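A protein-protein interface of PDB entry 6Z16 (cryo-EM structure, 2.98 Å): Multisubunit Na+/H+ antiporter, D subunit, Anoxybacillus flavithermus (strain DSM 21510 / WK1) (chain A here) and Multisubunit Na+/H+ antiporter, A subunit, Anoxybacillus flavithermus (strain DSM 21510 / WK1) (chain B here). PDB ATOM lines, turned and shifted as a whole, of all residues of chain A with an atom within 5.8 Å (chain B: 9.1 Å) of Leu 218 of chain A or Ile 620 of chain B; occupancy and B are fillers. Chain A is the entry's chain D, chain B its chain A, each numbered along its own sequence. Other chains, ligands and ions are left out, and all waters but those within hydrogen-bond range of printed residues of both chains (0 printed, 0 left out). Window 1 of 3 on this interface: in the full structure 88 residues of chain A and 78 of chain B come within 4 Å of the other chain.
The indole nitrogen of Trp 228 of chain A is in hydrogen-bond range of the backbone carbonyl oxygen of Leu 225 of chain A.
O of Leu 218 of chain A is in hydrogen-bond range of NE1 of Trp 228 of chain A (3.2 Å).
OG of Ser 169 of chain A lies within hydrogen-bond range of O of Val 165 of chain A, at 3.4 Å.
The backbone carbonyl oxygen (O) of Tyr 619 of chain B sits at hydrogen-bond distance from the side-chain hydroxyl (OG) of Ser 623 of chain B, 2.8 Å away.
Of the printed residues of chain A, Ile 620 of chain B touches Leu 218 and Leu 225.
Gly 217 of chain A touches none of the printed residues of chain B.
No residue of chain B comes within 4 Å of Gly 220 of chain A.
Of the printed residues of chain B, Pro 224 of chain A touches Ser 623 (3.4 Å).
Of the printed residues of chain A, Leu 624 of chain B touches Ile 214 (3.7 Å).
Of the printed residues of chain B, Leu 225 of chain A touches Ile 620.
Of the printed residues of chain A, Leu 617 of chain B touches Ile 168 (3.7 Å).
Printed residues of chain B within 4 Å of Ile 168 of chain A: Leu 617.
Phe 216 of chain A touches none of the printed residues of chain B.
The nearest residue of chain B that does not touch Leu 218 of chain A is Leu 624 of chain B (6.7 Å).
Among the printed residues, merely in contact across the chains: Pro 224 of chain A with Ser 623 of chain B, Phe 227 of chain A with Tyr 616 of chain B, Val 165 of chain A with Met 613 of chain B, Ile 214 of chain A with Leu 624 of chain B, Ile 168 of chain A with Leu 617 of chain B, Leu 218 of chain A with Ile 620 of chain B, Phe 227 of chain A with Tyr 619 of chain B and Leu 225 of chain A with Ile 620 of chain B.
Of the 19 printed residues of chain A, 7 touch a printed residue of chain B.
Hydrophobic or aromatic side chains of chain A within 4 Å of the printed part of chain B: Val 165, Ile 168, Ile 214, Leu 218, Pro 224, Leu 225 and Phe 227.
Hydrophobic or aromatic side chains of chain B within 4 Å of the printed part of chain A: Met 613, Tyr 616, Leu 617, Tyr 619, Ile 620 and Leu 624.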
ATOM      1  N   VAL A 165     -13.573  21.036  14.038  1.00  0.00           N
ATOM      2  CA  VAL A 165     -14.579  21.692  13.197  1.00  0.00           C
ATOM      3  C   VAL A 165     -15.634  22.392  14.044  1.00  0.00           C
ATOM      4  O   VAL A 165     -16.024  23.539  13.764  1.00  0.00           O
ATOM      5  CB  VAL A 165     -15.231  20.672  12.247  1.00  0.00           C
ATOM      6  CG1 VAL A 165     -16.294  21.337  11.389  1.00  0.00           C
ATOM      7  CG2 VAL A 165     -14.206  20.058  11.391  1.00  0.00           C
ATOM      8  N   ASN A 166     -16.093  21.732  15.108  1.00  0.00           N
ATOM      9  CA  ASN A 166     -17.177  22.328  15.880  1.00  0.00           C
ATOM     10  C   ASN A 166     -16.703  23.484  16.750  1.00  0.00           C
ATOM     11  O   ASN A 166     -17.489  24.393  17.034  1.00  0.00           O
ATOM     12  CB  ASN A 166     -17.858  21.261  16.712  1.00  0.00           C
ATOM     13  CG  ASN A 166     -18.625  20.294  15.872  1.00  0.00           C
ATOM     14  OD1 ASN A 166     -19.371  20.685  14.977  1.00  0.00           O
ATOM     15  ND2 ASN A 166     -18.419  19.018  16.123  1.00  0.00           N
ATOM     16  N   ILE A 168     -14.405  25.667  15.673  1.00  0.00           N
ATOM     17  CA  ILE A 168     -14.386  26.768  14.706  1.00  0.00           C
ATOM     18  C   ILE A 168     -15.794  27.307  14.450  1.00  0.00           C
ATOM     19  O   ILE A 168     -16.020  28.527  14.465  1.00  0.00           O
ATOM     20  CB  ILE A 168     -13.695  26.310  13.411  1.00  0.00           C
ATOM     21  CG1 ILE A 168     -12.227  26.015  13.693  1.00  0.00           C
ATOM     22  CG2 ILE A 168     -13.823  27.349  12.326  1.00  0.00           C
ATOM     23  CD1 ILE A 168     -11.533  25.343  12.566  1.00  0.00           C
ATOM     24  N   SER A 169     -16.771  26.412  14.293  1.00  0.00           N
ATOM     25  CA  SER A 169     -18.139  26.863  14.040  1.00  0.00           C
ATOM     26  C   SER A 169     -18.780  27.510  15.270  1.00  0.00           C
ATOM     27  O   SER A 169     -19.622  28.407  15.130  1.00  0.00           O
ATOM     28  CB  SER A 169     -18.982  25.695  13.544  1.00  0.00           C
ATOM     29  OG  SER A 169     -19.084  24.689  14.532  1.00  0.00           O
ATOM     30  N   LEU A 172     -17.553  31.015  15.278  1.00  0.00           N
ATOM     31  CA  LEU A 172     -18.266  31.762  14.245  1.00  0.00           C
ATOM     32  C   LEU A 172     -19.688  32.118  14.668  1.00  0.00           C
ATOM     33  O   LEU A 172     -20.193  33.188  14.301  1.00  0.00           O
ATOM     34  CB  LEU A 172     -18.265  30.970  12.942  1.00  0.00           C
ATOM     35  CG  LEU A 172     -16.888  30.852  12.282  1.00  0.00           C
ATOM     36  CD1 LEU A 172     -16.910  29.870  11.135  1.00  0.00           C
ATOM     37  CD2 LEU A 172     -16.424  32.212  11.801  1.00  0.00           C
ATOM     38  N   ILE A 213     -26.143  31.256   7.696  1.00  0.00           N
ATOM     39  CA  ILE A 213     -26.144  30.123   6.766  1.00  0.00           C
ATOM     40  C   ILE A 213     -24.855  29.330   6.897  1.00  0.00           C
ATOM     41  O   ILE A 213     -24.879  28.097   6.968  1.00  0.00           O
ATOM     42  CB  ILE A 213     -26.338  30.592   5.313  1.00  0.00           C
ATOM     43  CG1 ILE A 213     -27.708  31.197   5.102  1.00  0.00           C
ATOM     44  CG2 ILE A 213     -26.163  29.449   4.336  1.00  0.00           C
ATOM     45  CD1 ILE A 213     -27.835  31.874   3.769  1.00  0.00           C
ATOM     46  N   ILE A 214     -23.720  30.026   6.971  1.00  0.00           N
ATOM     47  CA  ILE A 214     -22.429  29.343   7.059  1.00  0.00           C
ATOM     48  C   ILE A 214     -22.293  28.596   8.385  1.00  0.00           C
ATOM     49  O   ILE A 214     -21.836  27.445   8.416  1.00  0.00           O
ATOM     50  CB  ILE A 214     -21.286  30.349   6.840  1.00  0.00           C
ATOM     51  CG1 ILE A 214     -21.380  30.936   5.435  1.00  0.00           C
ATOM     52  CG2 ILE A 214     -19.933  29.682   7.016  1.00  0.00           C
ATOM     53  CD1 ILE A 214     -20.557  32.177   5.233  1.00  0.00           C
ATOM     54  N   VAL A 215     -22.758  29.203   9.484  1.00  0.00           N
ATOM     55  CA  VAL A 215     -22.675  28.556  10.797  1.00  0.00           C
ATOM     56  C   VAL A 215     -23.573  27.322  10.860  1.00  0.00           C
ATOM     57  O   VAL A 215     -23.120  26.215  11.184  1.00  0.00           O
ATOM     58  CB  VAL A 215     -23.031  29.552  11.914  1.00  0.00           C
ATOM     59  CG1 VAL A 215     -23.131  28.826  13.234  1.00  0.00           C
ATOM     60  CG2 VAL A 215     -21.991  30.640  12.008  1.00  0.00           C
ATOM     61  N   PHE A 216     -24.856  27.489  10.527  1.00  0.00           N
ATOM     62  CA  PHE A 216     -25.805  26.388  10.620  1.00  0.00           C
ATOM     63  C   PHE A 216     -25.573  25.325   9.557  1.00  0.00           C
ATOM     64  O   PHE A 216     -25.998  24.184   9.744  1.00  0.00           O
ATOM     65  CB  PHE A 216     -27.225  26.928  10.525  1.00  0.00           C
ATOM     66  CG  PHE A 216     -27.636  27.772  11.695  1.00  0.00           C
ATOM     67  CD1 PHE A 216     -27.020  27.639  12.926  1.00  0.00           C
ATOM     68  CD2 PHE A 216     -28.620  28.732  11.550  1.00  0.00           C
ATOM     69  CE1 PHE A 216     -27.395  28.428  13.992  1.00  0.00           C
ATOM     70  CE2 PHE A 216     -28.996  29.525  12.612  1.00  0.00           C
ATOM     71  CZ  PHE A 216     -28.381  29.372  13.833  1.00  0.00           C
ATOM     72  N   GLY A 217     -24.899  25.663   8.456  1.00  0.00           N
ATOM     73  CA  GLY A 217     -24.473  24.662   7.505  1.00  0.00           C
ATOM     74  C   GLY A 217     -23.192  23.963   7.879  1.00  0.00           C
ATOM     75  O   GLY A 217     -22.916  22.879   7.361  1.00  0.00           O
ATOM     76  N   LEU A 218     -22.380  24.573   8.737  1.00  0.00           N
ATOM     77  CA  LEU A 218     -21.365  23.789   9.422  1.00  0.00           C
ATOM     78  C   LEU A 218     -21.993  22.839  10.432  1.00  0.00           C
ATOM     79  O   LEU A 218     -21.459  21.748  10.664  1.00  0.00           O
ATOM     80  CB  LEU A 218     -20.355  24.711  10.099  1.00  0.00           C
ATOM     81  CG  LEU A 218     -19.344  25.353   9.158  1.00  0.00           C
ATOM     82  CD1 LEU A 218     -18.569  26.440   9.863  1.00  0.00           C
ATOM     83  CD2 LEU A 218     -18.406  24.269   8.661  1.00  0.00           C
ATOM     84  N   LYS A 219     -23.124  23.226  11.028  1.00  0.00           N
ATOM     85  CA  LYS A 219     -23.805  22.334  11.967  1.00  0.00           C
ATOM     86  C   LYS A 219     -24.436  21.146  11.245  1.00  0.00           C
ATOM     87  O   LYS A 219     -24.078  19.991  11.498  1.00  0.00           O
ATOM     88  CB  LYS A 219     -24.858  23.106  12.761  1.00  0.00           C
ATOM     89  CG  LYS A 219     -24.298  24.251  13.577  1.00  0.00           C
ATOM     90  CD  LYS A 219     -23.314  23.757  14.619  1.00  0.00           C
ATOM     91  CE  LYS A 219     -22.924  24.871  15.573  1.00  0.00           C
ATOM     92  NZ  LYS A 219     -22.135  25.924  14.894  1.00  0.00           N
ATOM     93  N   GLY A 220     -25.383  21.408  10.348  1.00  0.00           N
ATOM     94  CA  GLY A 220     -25.949  20.383   9.498  1.00  0.00           C
ATOM     95  C   GLY A 220     -25.357  20.500   8.111  1.00  0.00           C
ATOM     96  O   GLY A 220     -25.450  21.548   7.483  1.00  0.00           O
ATOM     97  N   ALA A 221     -24.774  19.402   7.626  1.00  0.00           N
ATOM     98  CA  ALA A 221     -23.783  19.435   6.548  1.00  0.00           C
ATOM     99  C   ALA A 221     -24.396  19.857   5.215  1.00  0.00           C
ATOM    100  O   ALA A 221     -25.103  19.079   4.570  1.00  0.00           O
ATOM    101  CB  ALA A 221     -23.129  18.068   6.415  1.00  0.00           C
ATOM    102  N   ILE A 222     -24.102  21.085   4.804  1.00  0.00           N
ATOM    103  CA  ILE A 222     -24.462  21.609   3.499  1.00  0.00           C
ATOM    104  C   ILE A 222     -23.196  21.580   2.648  1.00  0.00           C
ATOM    105  O   ILE A 222     -22.085  21.533   3.163  1.00  0.00           O
ATOM    106  CB  ILE A 222     -25.044  23.046   3.631  1.00  0.00           C
ATOM    107  CG1 ILE A 222     -26.145  23.077   4.677  1.00  0.00           C
ATOM    108  CG2 ILE A 222     -25.682  23.557   2.364  1.00  0.00           C
ATOM    109  CD1 ILE A 222     -27.278  22.156   4.400  1.00  0.00           C
ATOM    110  N   PRO A 224     -20.835  23.925   0.566  1.00  0.00           N
ATOM    111  CA  PRO A 224     -19.532  23.266   0.666  1.00  0.00           C
ATOM    112  C   PRO A 224     -18.978  23.234   2.084  1.00  0.00           C
ATOM    113  O   PRO A 224     -17.819  23.569   2.301  1.00  0.00           O
ATOM    114  CB  PRO A 224     -18.650  24.135  -0.216  1.00  0.00           C
ATOM    115  CG  PRO A 224     -19.207  25.485  -0.020  1.00  0.00           C
ATOM    116  CD  PRO A 224     -20.685  25.336   0.172  1.00  0.00           C
ATOM    117  N   LEU A 225     -19.812  22.846   3.045  1.00  0.00           N
ATOM    118  CA  LEU A 225     -19.443  22.837   4.454  1.00  0.00           C
ATOM    119  C   LEU A 225     -19.613  21.451   5.060  1.00  0.00           C
ATOM    120  O   LEU A 225     -19.768  21.325   6.276  1.00  0.00           O
ATOM    121  CB  LEU A 225     -20.297  23.857   5.206  1.00  0.00           C
ATOM    122  CG  LEU A 225     -20.205  25.291   4.694  1.00  0.00           C
ATOM    123  CD1 LEU A 225     -21.248  26.164   5.338  1.00  0.00           C
ATOM    124  CD2 LEU A 225     -18.823  25.844   4.942  1.00  0.00           C
ATOM    125  N   PHE A 227     -17.598  18.657   4.798  1.00  0.00           N
ATOM    126  CA  PHE A 227     -16.450  17.781   4.600  1.00  0.00           C
ATOM    127  C   PHE A 227     -16.026  17.035   5.858  1.00  0.00           C
ATOM    128  O   PHE A 227     -15.250  16.077   5.764  1.00  0.00           O
ATOM    129  CB  PHE A 227     -15.273  18.605   4.083  1.00  0.00           C
ATOM    130  CG  PHE A 227     -15.497  19.212   2.730  1.00  0.00           C
ATOM    131  CD1 PHE A 227     -15.265  18.482   1.577  1.00  0.00           C
ATOM    132  CD2 PHE A 227     -15.913  20.529   2.615  1.00  0.00           C
ATOM    133  CE1 PHE A 227     -15.455  19.046   0.337  1.00  0.00           C
ATOM    134  CE2 PHE A 227     -16.105  21.096   1.370  1.00  0.00           C
ATOM    135  CZ  PHE A 227     -15.878  20.350   0.235  1.00  0.00           C
ATOM    136  N   TRP A 228     -16.499  17.454   7.026  1.00  0.00           N
ATOM    137  CA  TRP A 228     -16.133  16.807   8.275  1.00  0.00           C
ATOM    138  C   TRP A 228     -16.895  15.518   8.530  1.00  0.00           C
ATOM    139  O   TRP A 228     -16.395  14.656   9.256  1.00  0.00           O
ATOM    140  CB  TRP A 228     -16.362  17.778   9.429  1.00  0.00           C
ATOM    141  CG  TRP A 228     -17.749  18.340   9.480  1.00  0.00           C
ATOM    142  CD1 TRP A 228     -18.194  19.465   8.862  1.00  0.00           C
ATOM    143  CD2 TRP A 228     -18.862  17.818  10.208  1.00  0.00           C
ATOM    144  NE1 TRP A 228     -19.518  19.673   9.148  1.00  0.00           N
ATOM    145  CE2 TRP A 228     -19.952  18.675   9.975  1.00  0.00           C
ATOM    146  CE3 TRP A 228     -19.041  16.711  11.036  1.00  0.00           C
ATOM    147  CZ2 TRP A 228     -21.204  18.455  10.533  1.00  0.00           C
ATOM    148  CZ3 TRP A 228     -20.285  16.490  11.579  1.00  0.00           C
ATOM    149  CH2 TRP A 228     -21.349  17.361  11.334  1.00  0.00           C
ATOM    150  N   MET B 613      -6.958  16.954   7.016  1.00  0.00           N
ATOM    151  CA  MET B 613      -7.823  17.951   7.629  1.00  0.00           C
ATOM    152  C   MET B 613      -7.481  19.359   7.153  1.00  0.00           C
ATOM    153  O   MET B 613      -8.365  20.230   7.106  1.00  0.00           O
ATOM    154  CB  MET B 613      -7.722  17.834   9.150  1.00  0.00           C
ATOM    155  CG  MET B 613      -8.754  18.639   9.877  1.00  0.00           C
ATOM    156  SD  MET B 613     -10.376  18.043   9.419  1.00  0.00           S
ATOM    157  CE  MET B 613     -11.228  19.595   9.388  1.00  0.00           C
ATOM    158  N   ARG B 614      -6.217  19.577   6.764  1.00  0.00           N
ATOM    159  CA  ARG B 614      -5.762  20.874   6.268  1.00  0.00           C
ATOM    160  C   ARG B 614      -6.522  21.292   5.021  1.00  0.00           C
ATOM    161  O   ARG B 614      -6.937  22.450   4.895  1.00  0.00           O
ATOM    162  CB  ARG B 614      -4.268  20.815   5.957  1.00  0.00           C
ATOM    163  CG  ARG B 614      -3.382  20.547   7.145  1.00  0.00           C
ATOM    164  CD  ARG B 614      -1.927  20.442   6.728  1.00  0.00           C
ATOM    165  NE  ARG B 614      -1.393  21.709   6.244  1.00  0.00           N
ATOM    166  CZ  ARG B 614      -0.181  21.854   5.721  1.00  0.00           C
ATOM    167  NH1 ARG B 614       0.624  20.808   5.614  1.00  0.00           N
ATOM    168  NH2 ARG B 614       0.231  23.044   5.312  1.00  0.00           N
ATOM    169  N   THR B 615      -6.744  20.345   4.106  1.00  0.00           N
ATOM    170  CA  THR B 615      -7.435  20.644   2.859  1.00  0.00           C
ATOM    171  C   THR B 615      -8.894  21.005   3.096  1.00  0.00           C
ATOM    172  O   THR B 615      -9.401  21.960   2.495  1.00  0.00           O
ATOM    173  CB  THR B 615      -7.316  19.460   1.906  1.00  0.00           C
ATOM    174  OG1 THR B 615      -7.865  18.295   2.527  1.00  0.00           O
ATOM    175  CG2 THR B 615      -5.866  19.201   1.579  1.00  0.00           C
ATOM    176  N   TYR B 616      -9.577  20.282   3.992  1.00  0.00           N
ATOM    177  CA  TYR B 616     -10.979  20.593   4.248  1.00  0.00           C
ATOM    178  C   TYR B 616     -11.122  21.922   4.967  1.00  0.00           C
ATOM    179  O   TYR B 616     -12.088  22.656   4.725  1.00  0.00           O
ATOM    180  CB  TYR B 616     -11.664  19.510   5.073  1.00  0.00           C
ATOM    181  CG  TYR B 616     -11.530  18.108   4.554  1.00  0.00           C
ATOM    182  CD1 TYR B 616     -11.936  17.780   3.269  1.00  0.00           C
ATOM    183  CD2 TYR B 616     -11.110  17.086   5.387  1.00  0.00           C
ATOM    184  CE1 TYR B 616     -11.836  16.491   2.808  1.00  0.00           C
ATOM    185  CE2 TYR B 616     -11.016  15.789   4.926  1.00  0.00           C
ATOM    186  CZ  TYR B 616     -11.383  15.502   3.640  1.00  0.00           C
ATOM    187  OH  TYR B 616     -11.293  14.211   3.184  1.00  0.00           O
ATOM    188  N   LEU B 617     -10.161  22.254   5.835  1.00  0.00           N
ATOM    189  CA  LEU B 617     -10.151  23.575   6.450  1.00  0.00           C
ATOM    190  C   LEU B 617      -9.925  24.668   5.416  1.00  0.00           C
ATOM    191  O   LEU B 617     -10.534  25.742   5.509  1.00  0.00           O
ATOM    192  CB  LEU B 617      -9.091  23.635   7.542  1.00  0.00           C
ATOM    193  CG  LEU B 617      -9.433  22.838   8.792  1.00  0.00           C
ATOM    194  CD1 LEU B 617      -8.251  22.787   9.719  1.00  0.00           C
ATOM    195  CD2 LEU B 617     -10.628  23.461   9.469  1.00  0.00           C
ATOM    196  N   MET B 618      -9.066  24.406   4.422  1.00  0.00           N
ATOM    197  CA  MET B 618      -8.886  25.348   3.319  1.00  0.00           C
ATOM    198  C   MET B 618     -10.182  25.562   2.549  1.00  0.00           C
ATOM    199  O   MET B 618     -10.517  26.701   2.204  1.00  0.00           O
ATOM    200  CB  MET B 618      -7.794  24.868   2.366  1.00  0.00           C
ATOM    201  CG  MET B 618      -6.376  24.945   2.890  1.00  0.00           C
ATOM    202  SD  MET B 618      -5.229  24.324   1.644  1.00  0.00           S
ATOM    203  CE  MET B 618      -3.684  24.293   2.546  1.00  0.00           C
ATOM    204  N   TYR B 619     -10.943  24.483   2.301  1.00  0.00           N
ATOM    205  CA  TYR B 619     -12.189  24.627   1.544  1.00  0.00           C
ATOM    206  C   TYR B 619     -13.235  25.404   2.336  1.00  0.00           C
ATOM    207  O   TYR B 619     -13.919  26.272   1.779  1.00  0.00           O
ATOM    208  CB  TYR B 619     -12.787  23.276   1.140  1.00  0.00           C
ATOM    209  CG  TYR B 619     -11.922  22.371   0.305  1.00  0.00           C
ATOM    210  CD1 TYR B 619     -11.407  22.789  -0.907  1.00  0.00           C
ATOM    211  CD2 TYR B 619     -11.752  21.041   0.660  1.00  0.00           C
ATOM    212  CE1 TYR B 619     -10.639  21.944  -1.682  1.00  0.00           C
ATOM    213  CE2 TYR B 619     -10.996  20.185  -0.108  1.00  0.00           C
ATOM    214  CZ  TYR B 619     -10.444  20.639  -1.277  1.00  0.00           C
ATOM    215  OH  TYR B 619      -9.696  19.780  -2.044  1.00  0.00           O
ATOM    216  N   ILE B 620     -13.355  25.118   3.636  1.00  0.00           N
ATOM    217  CA  ILE B 620     -14.339  25.801   4.474  1.00  0.00           C
ATOM    218  C   ILE B 620     -13.999  27.284   4.621  1.00  0.00           C
ATOM    219  O   ILE B 620     -14.874  28.151   4.482  1.00  0.00           O
ATOM    220  CB  ILE B 620     -14.442  25.096   5.840  1.00  0.00           C
ATOM    221  CG1 ILE B 620     -15.019  23.690   5.677  1.00  0.00           C
ATOM    222  CG2 ILE B 620     -15.289  25.898   6.808  1.00  0.00           C
ATOM    223  CD1 ILE B 620     -14.888  22.832   6.902  1.00  0.00           C
ATOM    224  N   PHE B 621     -12.720  27.597   4.871  1.00  0.00           N
ATOM    225  CA  PHE B 621     -12.284  28.985   5.007  1.00  0.00           C
ATOM    226  C   PHE B 621     -12.433  29.759   3.703  1.00  0.00           C
ATOM    227  O   PHE B 621     -12.872  30.918   3.714  1.00  0.00           O
ATOM    228  CB  PHE B 621     -10.836  29.010   5.483  1.00  0.00           C
ATOM    229  CG  PHE B 621     -10.667  28.720   6.943  1.00  0.00           C
ATOM    230  CD1 PHE B 621     -11.664  29.038   7.845  1.00  0.00           C
ATOM    231  CD2 PHE B 621      -9.528  28.086   7.407  1.00  0.00           C
ATOM    232  CE1 PHE B 621     -11.511  28.770   9.186  1.00  0.00           C
ATOM    233  CE2 PHE B 621      -9.376  27.800   8.743  1.00  0.00           C
ATOM    234  CZ  PHE B 621     -10.368  28.143   9.634  1.00  0.00           C
ATOM    235  N   THR B 622     -12.100  29.130   2.569  1.00  0.00           N
ATOM    236  CA  THR B 622     -12.219  29.796   1.279  1.00  0.00           C
ATOM    237  C   THR B 622     -13.677  30.050   0.921  1.00  0.00           C
ATOM    238  O   THR B 622     -14.014  31.120   0.402  1.00  0.00           O
ATOM    239  CB  THR B 622     -11.527  28.954   0.208  1.00  0.00           C
ATOM    240  OG1 THR B 622     -10.180  28.694   0.611  1.00  0.00           O
ATOM    241  CG2 THR B 622     -11.490  29.686  -1.107  1.00  0.00           C
ATOM    242  N   SER B 623     -14.562  29.102   1.243  1.00  0.00           N
ATOM    243  CA  SER B 623     -15.984  29.287   0.977  1.00  0.00           C
ATOM    244  C   SER B 623     -16.583  30.377   1.859  1.00  0.00           C
ATOM    245  O   SER B 623     -17.417  31.166   1.396  1.00  0.00           O
ATOM    246  CB  SER B 623     -16.713  27.966   1.187  1.00  0.00           C
ATOM    247  OG  SER B 623     -16.212  26.976   0.308  1.00  0.00           O
ATOM    248  N   LEU B 624     -16.160  30.429   3.129  1.00  0.00           N
ATOM    249  CA  LEU B 624     -16.543  31.503   4.046  1.00  0.00           C
ATOM    250  C   LEU B 624     -16.161  32.873   3.497  1.00  0.00           C
ATOM    251  O   LEU B 624     -17.003  33.784   3.409  1.00  0.00           O
ATOM    252  CB  LEU B 624     -15.860  31.262   5.391  1.00  0.00           C
ATOM    253  CG  LEU B 624     -15.944  32.266   6.541  1.00  0.00           C
ATOM    254  CD1 LEU B 624     -17.334  32.372   7.100  1.00  0.00           C
ATOM    255  CD2 LEU B 624     -14.959  31.885   7.626  1.00  0.00           C
ATOM    256  N   VAL B 625     -14.889  33.016   3.099  1.00  0.00           N
ATOM    257  CA  VAL B 625     -14.367  34.270   2.556  1.00  0.00           C
ATOM    258  C   VAL B 625     -15.100  34.666   1.281  1.00  0.00           C
ATOM    259  O   VAL B 625     -15.504  35.825   1.121  1.00  0.00           O
ATOM    260  CB  VAL B 625     -12.851  34.137   2.329  1.00  0.00           C
ATOM    261  CG1 VAL B 625     -12.318  35.279   1.514  1.00  0.00           C
ATOM    262  CG2 VAL B 625     -12.154  34.124   3.643  1.00  0.00           C
ATOM    263  N   ALA B 626     -15.324  33.701   0.382  1.00  0.00           N
ATOM    264  CA  ALA B 626     -15.948  33.986  -0.904  1.00  0.00           C
ATOM    265  C   ALA B 626     -17.393  34.430  -0.741  1.00  0.00           C
ATOM    266  O   ALA B 626     -17.811  35.427  -1.342  1.00  0.00           O
ATOM    267  CB  ALA B 626     -15.866  32.758  -1.804  1.00  0.00           C
ATOM    268  N   LEU B 627     -18.162  33.723   0.096  1.00  0.00           N
ATOM    269  CA  LEU B 627     -19.565  34.079   0.290  1.00  0.00           C
ATOM    270  C   LEU B 627     -19.714  35.428   0.977  1.00  0.00           C
ATOM    271  O   LEU B 627     -20.538  36.251   0.551  1.00  0.00           O
ATOM    272  CB  LEU B 627     -20.281  32.989   1.082  1.00  0.00           C
ATOM    273  CG  LEU B 627     -20.532  31.679   0.339  1.00  0.00           C
ATOM    274  CD1 LEU B 627     -21.051  30.616   1.276  1.00  0.00           C
ATOM    275  CD2 LEU B 627     -21.515  31.918  -0.782  1.00  0.00           C
ATOM    276  N   LEU B 628     -18.886  35.706   1.991  1.00  0.00           N
ATOM    277  CA  LEU B 628     -19.020  36.979   2.693  1.00  0.00           C
ATOM    278  C   LEU B 628     -18.560  38.155   1.836  1.00  0.00           C
ATOM    279  O   LEU B 628     -19.228  39.197   1.810  1.00  0.00           O
ATOM    280  CB  LEU B 628     -18.258  36.931   4.012  1.00  0.00           C
ATOM    281  CG  LEU B 628     -18.901  36.031   5.060  1.00  0.00           C
ATOM    282  CD1 LEU B 628     -18.006  35.928   6.264  1.00  0.00           C
ATOM    283  CD2 LEU B 628     -20.249  36.590   5.450  1.00  0.00           C
ATOM    284  N   VAL B 739      -5.271  32.987   2.639  1.00  0.00           N
ATOM    285  CA  VAL B 739      -6.555  32.643   3.248  1.00  0.00           C
ATOM    286  C   VAL B 739      -6.692  33.285   4.626  1.00  0.00           C
ATOM    287  O   VAL B 739      -7.749  33.827   4.967  1.00  0.00           O
ATOM    288  CB  VAL B 739      -6.714  31.110   3.298  1.00  0.00           C
ATOM    289  CG1 VAL B 739      -7.851  30.703   4.182  1.00  0.00           C
ATOM    290  CG2 VAL B 739      -6.988  30.578   1.915  1.00  0.00           C
ATOM    291  N   VAL B 743      -9.476  36.033   5.785  1.00  0.00           N
ATOM    292  CA  VAL B 743     -10.381  35.784   6.913  1.00  0.00           C
ATOM    293  C   VAL B 743     -10.357  36.952   7.896  1.00  0.00           C
ATOM    294  O   VAL B 743     -11.411  37.471   8.304  1.00  0.00           O
ATOM    295  CB  VAL B 743     -10.010  34.458   7.606  1.00  0.00           C
ATOM    296  CG1 VAL B 743     -10.696  34.333   8.919  1.00  0.00           C
ATOM    297  CG2 VAL B 743     -10.411  33.280   6.762  1.00  0.00           C
